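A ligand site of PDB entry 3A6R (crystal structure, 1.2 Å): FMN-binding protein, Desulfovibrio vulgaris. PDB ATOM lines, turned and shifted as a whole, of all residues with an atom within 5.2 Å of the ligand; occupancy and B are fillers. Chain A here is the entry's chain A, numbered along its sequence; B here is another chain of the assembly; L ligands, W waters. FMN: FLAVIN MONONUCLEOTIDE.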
ATOM      1  N   VAL A  15       1.086  20.561   0.808  1.00  0.00           N
ATOM      2  CA  VAL A  15       1.058  20.132  -0.590  1.00  0.00           C
ATOM      3  C   VAL A  15       0.049  21.014  -1.355  1.00  0.00           C
ATOM      4  O   VAL A  15      -1.116  21.123  -0.977  1.00  0.00           O
ATOM      5  CB  VAL A  15       0.669  18.638  -0.697  1.00  0.00           C
ATOM      6  CG1 VAL A  15       0.527  18.246  -2.139  1.00  0.00           C
ATOM      7  CG2 VAL A  15       1.676  17.784   0.022  1.00  0.00           C
ATOM      8  N   HIS A  27      -5.963  16.756 -15.406  1.00  0.00           N
ATOM      9  CA  HIS A  27      -4.680  16.306 -14.868  1.00  0.00           C
ATOM     10  C   HIS A  27      -4.450  17.075 -13.579  1.00  0.00           C
ATOM     11  O   HIS A  27      -5.032  18.148 -13.377  1.00  0.00           O
ATOM     12  CB  HIS A  27      -3.538  16.529 -15.867  1.00  0.00           C
ATOM     13  CG  HIS A  27      -2.272  15.844 -15.470  1.00  0.00           C
ATOM     14  ND1 HIS A  27      -2.273  14.554 -14.990  1.00  0.00           N
ATOM     15  CD2 HIS A  27      -0.996  16.278 -15.412  1.00  0.00           C
ATOM     16  CE1 HIS A  27      -1.036  14.209 -14.671  1.00  0.00           C
ATOM     17  NE2 HIS A  27      -0.234  15.233 -14.937  1.00  0.00           N
ATOM     18  N   VAL A  29      -1.276  17.919 -10.627  1.00  0.00           N
ATOM     19  CA  VAL A  29       0.123  17.858 -10.175  1.00  0.00           C
ATOM     20  C   VAL A  29       0.287  18.670  -8.914  1.00  0.00           C
ATOM     21  O   VAL A  29      -0.648  19.343  -8.475  1.00  0.00           O
ATOM     22  CB  VAL A  29       1.105  18.317 -11.275  1.00  0.00           C
ATOM     23  CG1 VAL A  29       1.012  17.456 -12.529  1.00  0.00           C
ATOM     24  CG2 VAL A  29       0.931  19.826 -11.594  1.00  0.00           C
ATOM     25  N   ASN A  30       1.494  18.647  -8.370  1.00  0.00           N
ATOM     26  CA  ASN A  30       1.763  19.256  -7.078  1.00  0.00           C
ATOM     27  C   ASN A  30       2.977  20.149  -7.046  1.00  0.00           C
ATOM     28  O   ASN A  30       3.875  20.063  -7.893  1.00  0.00           O
ATOM     29  CB  ASN A  30       1.924  18.166  -6.011  1.00  0.00           C
ATOM     30  CG  ASN A  30       0.709  17.291  -5.885  1.00  0.00           C
ATOM     31  OD1 ASN A  30       0.752  16.093  -6.202  1.00  0.00           O
ATOM     32  ND2 ASN A  30      -0.394  17.860  -5.431  1.00  0.00           N
ATOM     33  N   THR A  31       2.976  21.021  -6.033  1.00  0.00           N
ATOM     34  CA  THR A  31       4.184  21.640  -5.535  1.00  0.00           C
ATOM     35  C   THR A  31       4.053  21.722  -4.016  1.00  0.00           C
ATOM     36  O   THR A  31       3.113  21.146  -3.427  1.00  0.00           O
ATOM     37  CB  THR A  31       4.495  22.984  -6.243  1.00  0.00           C
ATOM     38  OG1 THR A  31       5.788  23.458  -5.858  1.00  0.00           O
ATOM     39  CG2 THR A  31       3.482  24.061  -5.935  1.00  0.00           C
ATOM     40  N   TRP A  32       4.973  22.439  -3.371  1.00  0.00           N
ATOM     41  CA  TRP A  32       4.944  22.650  -1.919  1.00  0.00           C
ATOM     42  C   TRP A  32       4.505  24.053  -1.576  1.00  0.00           C
ATOM     43  O   TRP A  32       4.839  25.008  -2.318  1.00  0.00           O
ATOM     44  CB  TRP A  32       6.314  22.401  -1.322  1.00  0.00           C
ATOM     45  CG  TRP A  32       6.872  21.024  -1.464  1.00  0.00           C
ATOM     46  CD1 TRP A  32       7.909  20.636  -2.257  1.00  0.00           C
ATOM     47  CD2 TRP A  32       6.469  19.857  -0.730  1.00  0.00           C
ATOM     48  NE1 TRP A  32       8.163  19.292  -2.082  1.00  0.00           N
ATOM     49  CE2 TRP A  32       7.310  18.792  -1.143  1.00  0.00           C
ATOM     50  CE3 TRP A  32       5.493  19.608   0.238  1.00  0.00           C
ATOM     51  CZ2 TRP A  32       7.185  17.501  -0.633  1.00  0.00           C
ATOM     52  CZ3 TRP A  32       5.377  18.319   0.759  1.00  0.00           C
ATOM     53  CH2 TRP A  32       6.214  17.280   0.310  1.00  0.00           C
ATOM     54  N   TYR A  35       7.255  26.538  -1.786  1.00  0.00           N
ATOM     55  CA  TYR A  35       7.852  26.871  -3.078  1.00  0.00           C
ATOM     56  C   TYR A  35       7.142  28.016  -3.774  1.00  0.00           C
ATOM     57  O   TYR A  35       7.710  28.605  -4.701  1.00  0.00           O
ATOM     58  CB  TYR A  35       7.839  25.649  -3.988  1.00  0.00           C
ATOM     59  CG  TYR A  35       8.860  24.560  -3.734  1.00  0.00           C
ATOM     60  CD1 TYR A  35       9.634  24.521  -2.567  1.00  0.00           C
ATOM     61  CD2 TYR A  35       9.018  23.553  -4.667  1.00  0.00           C
ATOM     62  CE1 TYR A  35      10.571  23.488  -2.391  1.00  0.00           C
ATOM     63  CE2 TYR A  35       9.954  22.551  -4.486  1.00  0.00           C
ATOM     64  CZ  TYR A  35      10.708  22.520  -3.349  1.00  0.00           C
ATOM     65  OH  TYR A  35      11.642  21.513  -3.148  1.00  0.00           O
ATOM     66  N   VAL A  46       5.381  29.187  -9.616  1.00  0.00           N
ATOM     67  CA  VAL A  46       5.736  27.844  -9.196  1.00  0.00           C
ATOM     68  C   VAL A  46       7.005  27.423  -9.944  1.00  0.00           C
ATOM     69  O   VAL A  46       7.053  27.543 -11.164  1.00  0.00           O
ATOM     70  CB  VAL A  46       4.616  26.847  -9.557  1.00  0.00           C
ATOM     71  CG1 VAL A  46       5.000  25.414  -9.183  1.00  0.00           C
ATOM     72  CG2 VAL A  46       3.263  27.234  -8.947  1.00  0.00           C
ATOM     73  N   PRO A  47       8.028  26.909  -9.258  1.00  0.00           N
ATOM     74  CA  PRO A  47       9.170  26.356  -9.982  1.00  0.00           C
ATOM     75  C   PRO A  47       8.806  25.055 -10.683  1.00  0.00           C
ATOM     76  O   PRO A  47       8.251  24.139 -10.065  1.00  0.00           O
ATOM     77  CB  PRO A  47      10.198  26.103  -8.875  1.00  0.00           C
ATOM     78  CG  PRO A  47       9.354  25.822  -7.645  1.00  0.00           C
ATOM     79  CD  PRO A  47       8.145  26.729  -7.789  1.00  0.00           C
ATOM     80  N   VAL A  48       9.159  24.971 -11.968  1.00  0.00           N
ATOM     81  CA  VAL A  48       8.773  23.848 -12.809  1.00  0.00           C
ATOM     82  C   VAL A  48       9.995  22.985 -13.107  1.00  0.00           C
ATOM     83  O   VAL A  48      10.959  23.459 -13.744  1.00  0.00           O
ATOM     84  CB  VAL A  48       8.147  24.312 -14.145  1.00  0.00           C
ATOM     85  CG1 VAL A  48       7.907  23.117 -15.050  1.00  0.00           C
ATOM     86  CG2 VAL A  48       6.860  25.060 -13.907  1.00  0.00           C
ATOM     87  N   GLY A  49       9.967  21.739 -12.630  1.00  0.00           N
ATOM     88  CA  GLY A  49      10.963  20.748 -12.973  1.00  0.00           C
ATOM     89  C   GLY A  49      10.400  19.853 -14.052  1.00  0.00           C
ATOM     90  O   GLY A  49      10.948  19.775 -15.154  1.00  0.00           O
ATOM     91  N   GLY A  50       9.293  19.192 -13.761  1.00  0.00           N
ATOM     92  CA  GLY A  50       8.579  18.359 -14.728  1.00  0.00           C
ATOM     93  C   GLY A  50       7.471  19.141 -15.389  1.00  0.00           C
ATOM     94  O   GLY A  50       7.707  19.976 -16.246  1.00  0.00           O
ATOM     95  N   MET A  51       6.236  18.823 -14.980  1.00  0.00           N
ATOM     96  CA  MET A  51       5.021  19.501 -15.477  1.00  0.00           C
ATOM     97  C   MET A  51       4.959  19.559 -16.996  1.00  0.00           C
ATOM     98  O   MET A  51       4.486  20.540 -17.570  1.00  0.00           O
ATOM     99  CB  MET A  51       4.832  20.877 -14.810  1.00  0.00           C
ATOM    100  CG  MET A  51       4.720  20.774 -13.316  1.00  0.00           C
ATOM    101  SD  MET A  51       4.052  22.273 -12.586  1.00  0.00           S
ATOM    102  CE  MET A  51       4.154  21.866 -10.836  1.00  0.00           C
ATOM    103  N   HIS A  52       5.368  18.475 -17.635  1.00  0.00           N
ATOM    104  CA  HIS A  52       5.290  18.373 -19.086  1.00  0.00           C
ATOM    105  C   HIS A  52       3.857  18.143 -19.578  1.00  0.00           C
ATOM    106  O   HIS A  52       3.401  18.788 -20.524  1.00  0.00           O
ATOM    107  CB  HIS A  52       6.246  17.305 -19.591  1.00  0.00           C
ATOM    108  CG  HIS A  52       7.690  17.665 -19.399  1.00  0.00           C
ATOM    109  ND1 HIS A  52       8.288  18.678 -20.106  1.00  0.00           N
ATOM    110  CD2 HIS A  52       8.624  17.177 -18.563  1.00  0.00           C
ATOM    111  CE1 HIS A  52       9.559  18.784 -19.725  1.00  0.00           C
ATOM    112  NE2 HIS A  52       9.776  17.890 -18.788  1.00  0.00           N
ATOM    113  N   LYS A  53       3.139  17.244 -18.931  1.00  0.00           N
ATOM    114  CA  LYS A  53       1.741  17.041 -19.302  1.00  0.00           C
ATOM    115  C   LYS A  53       0.926  18.290 -18.953  1.00  0.00           C
ATOM    116  O   LYS A  53       0.062  18.743 -19.739  1.00  0.00           O
ATOM    117  CB  LYS A  53       1.168  15.821 -18.604  1.00  0.00           C
ATOM    118  CG  LYS A  53      -0.281  15.520 -18.968  1.00  0.00           C
ATOM    119  CD  LYS A  53      -0.775  14.212 -18.342  1.00  0.00           C
ATOM    120  CE  LYS A  53      -2.200  13.895 -18.748  1.00  0.00           C
ATOM    121  NZ  LYS A  53      -2.252  13.342 -20.112  1.00  0.00           N
ATOM    122  N   THR A  54       1.197  18.831 -17.777  1.00  0.00           N
ATOM    123  CA  THR A  54       0.562  20.067 -17.363  1.00  0.00           C
ATOM    124  C   THR A  54       0.786  21.177 -18.391  1.00  0.00           C
ATOM    125  O   THR A  54      -0.147  21.918 -18.706  1.00  0.00           O
ATOM    126  CB  THR A  54       1.116  20.448 -15.968  1.00  0.00           C
ATOM    127  OG1 THR A  54       0.710  19.435 -15.049  1.00  0.00           O
ATOM    128  CG2 THR A  54       0.635  21.808 -15.464  1.00  0.00           C
ATOM    129  N   GLU A  55       2.024  21.340 -18.851  1.00  0.00           N
ATOM    130  CA  GLU A  55       2.310  22.379 -19.826  1.00  0.00           C
ATOM    131  C   GLU A  55       1.561  22.137 -21.150  1.00  0.00           C
ATOM    132  O   GLU A  55       1.041  23.081 -21.745  1.00  0.00           O
ATOM    133  CB  GLU A  55       3.810  22.492 -20.057  1.00  0.00           C
ATOM    134  CG  GLU A  55       4.177  23.663 -20.968  1.00  0.00           C
ATOM    135  CD  GLU A  55       5.658  23.980 -21.027  1.00  0.00           C
ATOM    136  OE1 GLU A  55       5.984  25.080 -21.537  1.00  0.00           O
ATOM    137  OE2 GLU A  55       6.509  23.140 -20.647  1.00  0.00           O
ATOM    138  N   TRP A 106      17.040  23.137 -10.374  1.00  0.00           N
ATOM    139  CA  TRP A 106      16.333  22.110 -11.133  1.00  0.00           C
ATOM    140  C   TRP A 106      15.184  22.653 -11.978  1.00  0.00           C
ATOM    141  O   TRP A 106      14.609  21.928 -12.789  1.00  0.00           O
ATOM    142  CB  TRP A 106      15.828  21.030 -10.186  1.00  0.00           C
ATOM    143  CG  TRP A 106      15.065  21.554  -9.004  1.00  0.00           C
ATOM    144  CD1 TRP A 106      15.569  21.764  -7.760  1.00  0.00           C
ATOM    145  CD2 TRP A 106      13.664  21.878  -8.933  1.00  0.00           C
ATOM    146  NE1 TRP A 106      14.583  22.234  -6.936  1.00  0.00           N
ATOM    147  CE2 TRP A 106      13.399  22.290  -7.626  1.00  0.00           C
ATOM    148  CE3 TRP A 106      12.605  21.850  -9.863  1.00  0.00           C
ATOM    149  CZ2 TRP A 106      12.124  22.695  -7.199  1.00  0.00           C
ATOM    150  CZ3 TRP A 106      11.331  22.255  -9.436  1.00  0.00           C
ATOM    151  CH2 TRP A 106      11.101  22.659  -8.128  1.00  0.00           C
ATOM    152  N   LEU B  68      -1.955  13.750  -2.654  1.00  0.00           N
ATOM    153  CA  LEU B  68      -1.717  13.989  -1.244  1.00  0.00           C
ATOM    154  C   LEU B  68      -0.238  13.774  -0.990  1.00  0.00           C
ATOM    155  O   LEU B  68       0.448  13.148  -1.800  1.00  0.00           O
ATOM    156  CB  LEU B  68      -2.525  13.045  -0.348  1.00  0.00           C
ATOM    157  CG  LEU B  68      -2.180  11.554  -0.317  1.00  0.00           C
ATOM    158  CD1 LEU B  68      -2.824  10.898   0.897  1.00  0.00           C
ATOM    159  CD2 LEU B  68      -2.530  10.811  -1.592  1.00  0.00           C
ATOM    160  N   THR B  81       7.405  13.604   0.116  1.00  0.00           N
ATOM    161  CA  THR B  81       6.872  12.796  -0.953  1.00  0.00           C
ATOM    162  C   THR B  81       5.383  12.990  -1.100  1.00  0.00           C
ATOM    163  O   THR B  81       4.752  13.672  -0.294  1.00  0.00           O
ATOM    164  CB  THR B  81       7.228  11.298  -0.779  1.00  0.00           C
ATOM    165  OG1 THR B  81       6.966  10.616  -2.013  1.00  0.00           O
ATOM    166  CG2 THR B  81       6.419  10.653   0.289  1.00  0.00           C
ATOM    167  N   GLY B  82       4.846  12.421  -2.172  1.00  0.00           N
ATOM    168  CA  GLY B  82       3.402  12.434  -2.372  1.00  0.00           C
ATOM    169  C   GLY B  82       3.041  11.510  -3.499  1.00  0.00           C
ATOM    170  O   GLY B  82       3.912  10.884  -4.119  1.00  0.00           O
ATOM    171  N   PHE B  83       1.726  11.445  -3.774  1.00  0.00           N
ATOM    172  CA  PHE B  83       1.138  10.478  -4.674  1.00  0.00           C
ATOM    173  C   PHE B  83       0.104  11.090  -5.587  1.00  0.00           C
ATOM    174  O   PHE B  83      -0.635  11.998  -5.166  1.00  0.00           O
ATOM    175  CB  PHE B  83       0.436   9.352  -3.867  1.00  0.00           C
ATOM    176  CG  PHE B  83       1.389   8.427  -3.248  1.00  0.00           C
ATOM    177  CD1 PHE B  83       1.955   8.710  -2.025  1.00  0.00           C
ATOM    178  CD2 PHE B  83       1.797   7.271  -3.913  1.00  0.00           C
ATOM    179  CE1 PHE B  83       2.934   7.863  -1.481  1.00  0.00           C
ATOM    180  CE2 PHE B  83       2.744   6.421  -3.362  1.00  0.00           C
ATOM    181  CZ  PHE B  83       3.301   6.735  -2.154  1.00  0.00           C
ATOM    182  N   THR B 121       5.062  10.368  -6.871  1.00  0.00           N
ATOM    183  CA  THR B 121       5.537  11.327  -7.886  1.00  0.00           C
ATOM    184  C   THR B 121       6.714  12.172  -7.387  1.00  0.00           C
ATOM    185  O   THR B 121       7.128  13.118  -8.072  1.00  0.00           O
ATOM    186  CB  THR B 121       4.394  12.223  -8.333  1.00  0.00           C
ATOM    187  OG1 THR B 121       3.776  12.706  -7.146  1.00  0.00           O
ATOM    188  CG2 THR B 121       3.353  11.473  -9.149  1.00  0.00           C
ATOM    189  N   LEU B 122       7.283  11.805  -6.252  1.00  0.00           N
ATOM    190  CA  LEU B 122       8.465  12.470  -5.706  1.00  0.00           C
ATOM    191  C   LEU B 122       9.256  11.477  -4.870  1.00  0.00           C
ATOM    192  O   LEU B 122       8.628  10.660  -4.168  1.00  0.00           O
ATOM    193  CB  LEU B 122       8.028  13.684  -4.869  1.00  0.00           C
ATOM    194  CG  LEU B 122       9.070  14.559  -4.212  1.00  0.00           C
ATOM    195  CD1 LEU B 122      10.015  15.162  -5.225  1.00  0.00           C
ATOM    196  CD2 LEU B 122       8.384  15.682  -3.436  1.00  0.00           C
ATOM    197  OXT LEU B 122      10.530  11.515  -4.870  1.00  0.00           O
HETATM  198  N1  FMN L   1       7.072  19.029  -9.920  1.00  0.00           N
HETATM  199  C2  FMN L   1       7.509  20.258 -10.342  1.00  0.00           C
HETATM  200  O2  FMN L   1       7.777  20.438 -11.521  1.00  0.00           O
HETATM  201  N3  FMN L   1       7.715  21.286  -9.433  1.00  0.00           N
HETATM  202  C4  FMN L   1       7.499  21.121  -8.083  1.00  0.00           C
HETATM  203  O4  FMN L   1       7.684  22.100  -7.329  1.00  0.00           O
HETATM  204  C4A FMN L   1       7.047  19.874  -7.655  1.00  0.00           C
HETATM  205  N5  FMN L   1       6.814  19.649  -6.319  1.00  0.00           N
HETATM  206  C5A FMN L   1       6.157  18.500  -5.931  1.00  0.00           C
HETATM  207  C6  FMN L   1       5.702  18.387  -4.623  1.00  0.00           C
HETATM  208  C7  FMN L   1       5.028  17.267  -4.190  1.00  0.00           C
HETATM  209  C7M FMN L   1       4.529  17.194  -2.776  1.00  0.00           C
HETATM  210  C8  FMN L   1       4.842  16.213  -5.093  1.00  0.00           C
HETATM  211  C8M FMN L   1       4.120  14.931  -4.655  1.00  0.00           C
HETATM  212  C9  FMN L   1       5.282  16.310  -6.405  1.00  0.00           C
HETATM  213  C9A FMN L   1       5.942  17.469  -6.842  1.00  0.00           C
HETATM  214  N10 FMN L   1       6.364  17.629  -8.184  1.00  0.00           N
HETATM  215  C10 FMN L   1       6.835  18.848  -8.595  1.00  0.00           C
HETATM  216  C1' FMN L   1       6.025  16.630  -9.202  1.00  0.00           C
HETATM  217  C2' FMN L   1       4.705  17.012  -9.951  1.00  0.00           C
HETATM  218  O2' FMN L   1       3.579  16.895  -9.093  1.00  0.00           O
HETATM  219  C3' FMN L   1       4.517  16.182 -11.229  1.00  0.00           C
HETATM  220  O3' FMN L   1       4.381  14.811 -10.859  1.00  0.00           O
HETATM  221  C4' FMN L   1       5.664  16.310 -12.236  1.00  0.00           C
HETATM  222  O4' FMN L   1       6.060  17.677 -12.399  1.00  0.00           O
HETATM  223  C5' FMN L   1       5.225  15.804 -13.584  1.00  0.00           C
HETATM  224  O5' FMN L   1       4.197  16.681 -14.096  1.00  0.00           O
HETATM  225  P   FMN L   1       3.292  16.224 -15.364  1.00  0.00           P
HETATM  226  O1P FMN L   1       2.495  14.983 -14.894  1.00  0.00           O
HETATM  227  O2P FMN L   1       4.234  15.881 -16.535  1.00  0.00           O
HETATM  228  O3P FMN L   1       2.419  17.403 -15.668  1.00  0.00           O
HETATM  229  O   HOH W   1       2.181  12.554 -15.918  1.00  0.00           O
HETATM  230  O   HOH W   2      10.314  18.461 -10.672  1.00  0.00           O
HETATM  231  O   HOH W   3       4.295  13.512 -18.198  1.00  0.00           O
HETATM  232  O   HOH W   4       8.978  16.310 -11.395  1.00  0.00           O
HETATM  233  O   HOH W   5       2.484  13.755 -12.468  1.00  0.00           O
HETATM  234  O   HOH W   6       9.956  17.980  -7.801  1.00  0.00           O
HETATM  235  O   HOH W   7       6.398  12.939 -11.418  1.00  0.00           O
HETATM  236  O   HOH W   8       6.829  15.781 -16.812  1.00  0.00           O
HETATM  237  O   HOH W   9       2.245  14.744  -8.066  1.00  0.00           O
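Merely in contact with the ligand: Val 29 (3.4 Å), Trp 32 (3.4 Å), Tyr 35 (3.3 Å), Val 48 (3.7 Å), Trp 106 (3.6 Å), Gly 82 of chain B (3.5 Å), Thr 121 of chain B (3.4 Å) and Leu 122 of chain B (3.8 Å). Hydrophobic or aromatic side chains that line the ligand: His 27, Val 29, Trp 32, Tyr 35, Met 51, His 52, Trp 106 and Leu 122 of chain B. 18 residues have an atom within 4 Å of the ligand: His 27, Val 29, Asn 30, Thr 31, Trp 32, Tyr 35, Pro 47, Val 48, Gly 49, Gly 50, Met 51, His 52, Lys 53, Thr 54, Trp 106, Gly 82 of chain B, Thr 121 of chain B and Leu 122 of chain B. The nearest printed residue that does not touch the ligand is Val 15 (4.04 Å).
O2P of the ligand is in hydrogen-bond range of N of Lys 53. OG1 of Thr 31 lies within hydrogen-bond range of O4 of the ligand, at 2.8 Å. O3P of the ligand sits at hydrogen-bond distance from N of Thr 54 (2.8 Å). An oxygen (O2) of the ligand is in hydrogen-bond range of the backbone NH (N) of Gly 49 (2.8 Å). NE2 of His 27 is in hydrogen-bond range of O1P of the ligand. The backbone NH (N) of Gly 50 is in hydrogen-bond range of an oxygen (O2) of the ligand, at 3.0 Å. O4' of the ligand is in hydrogen-bond range of N of Met 51 (2.8 Å). O2' of the ligand sits at hydrogen-bond distance from N of Asn 30 (2.8 Å). O of Asn 30 lies close to O2' of the ligand (3.4 Å). The backbone carbonyl oxygen of Pro 47 lies within hydrogen-bond range of a nitrogen (N3) of the ligand, 3.0 Å away. The backbone NH of His 52 lies within hydrogen-bond range of an oxygen (O2P) of the ligand (3.0 Å). The side-chain hydroxyl (OG1) of Thr 54 is in hydrogen-bond range of an oxygen (O3P) of the ligand (2.7 Å).
O of Gly 82 of chain B is in hydrogen-bond range of N of Thr 121 of chain B (3.0 Å). The side-chain hydroxyl of Thr 81 of chain B is in hydrogen-bond range of the chain-end carboxylate of Leu 122 of chain B (2.7 Å).
Water W8 bridges an oxygen (O2P) of the ligand (2.6 Å) and the backbone NH of His 52 (3.2 Å). Water W9 lies within hydrogen-bond range of OG1 of Thr 121 of chain B (2.7 Å), O2' of the ligand (2.7 Å) and OD1 of Asn 30 (2.7 Å). Water W7 bridges an oxygen (O3') of the ligand (2.8 Å) and the backbone carbonyl oxygen of Thr 121 of chain B (3.4 Å). Water W2 lies within hydrogen-bond range of O2 of the ligand and N of Gly 50.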
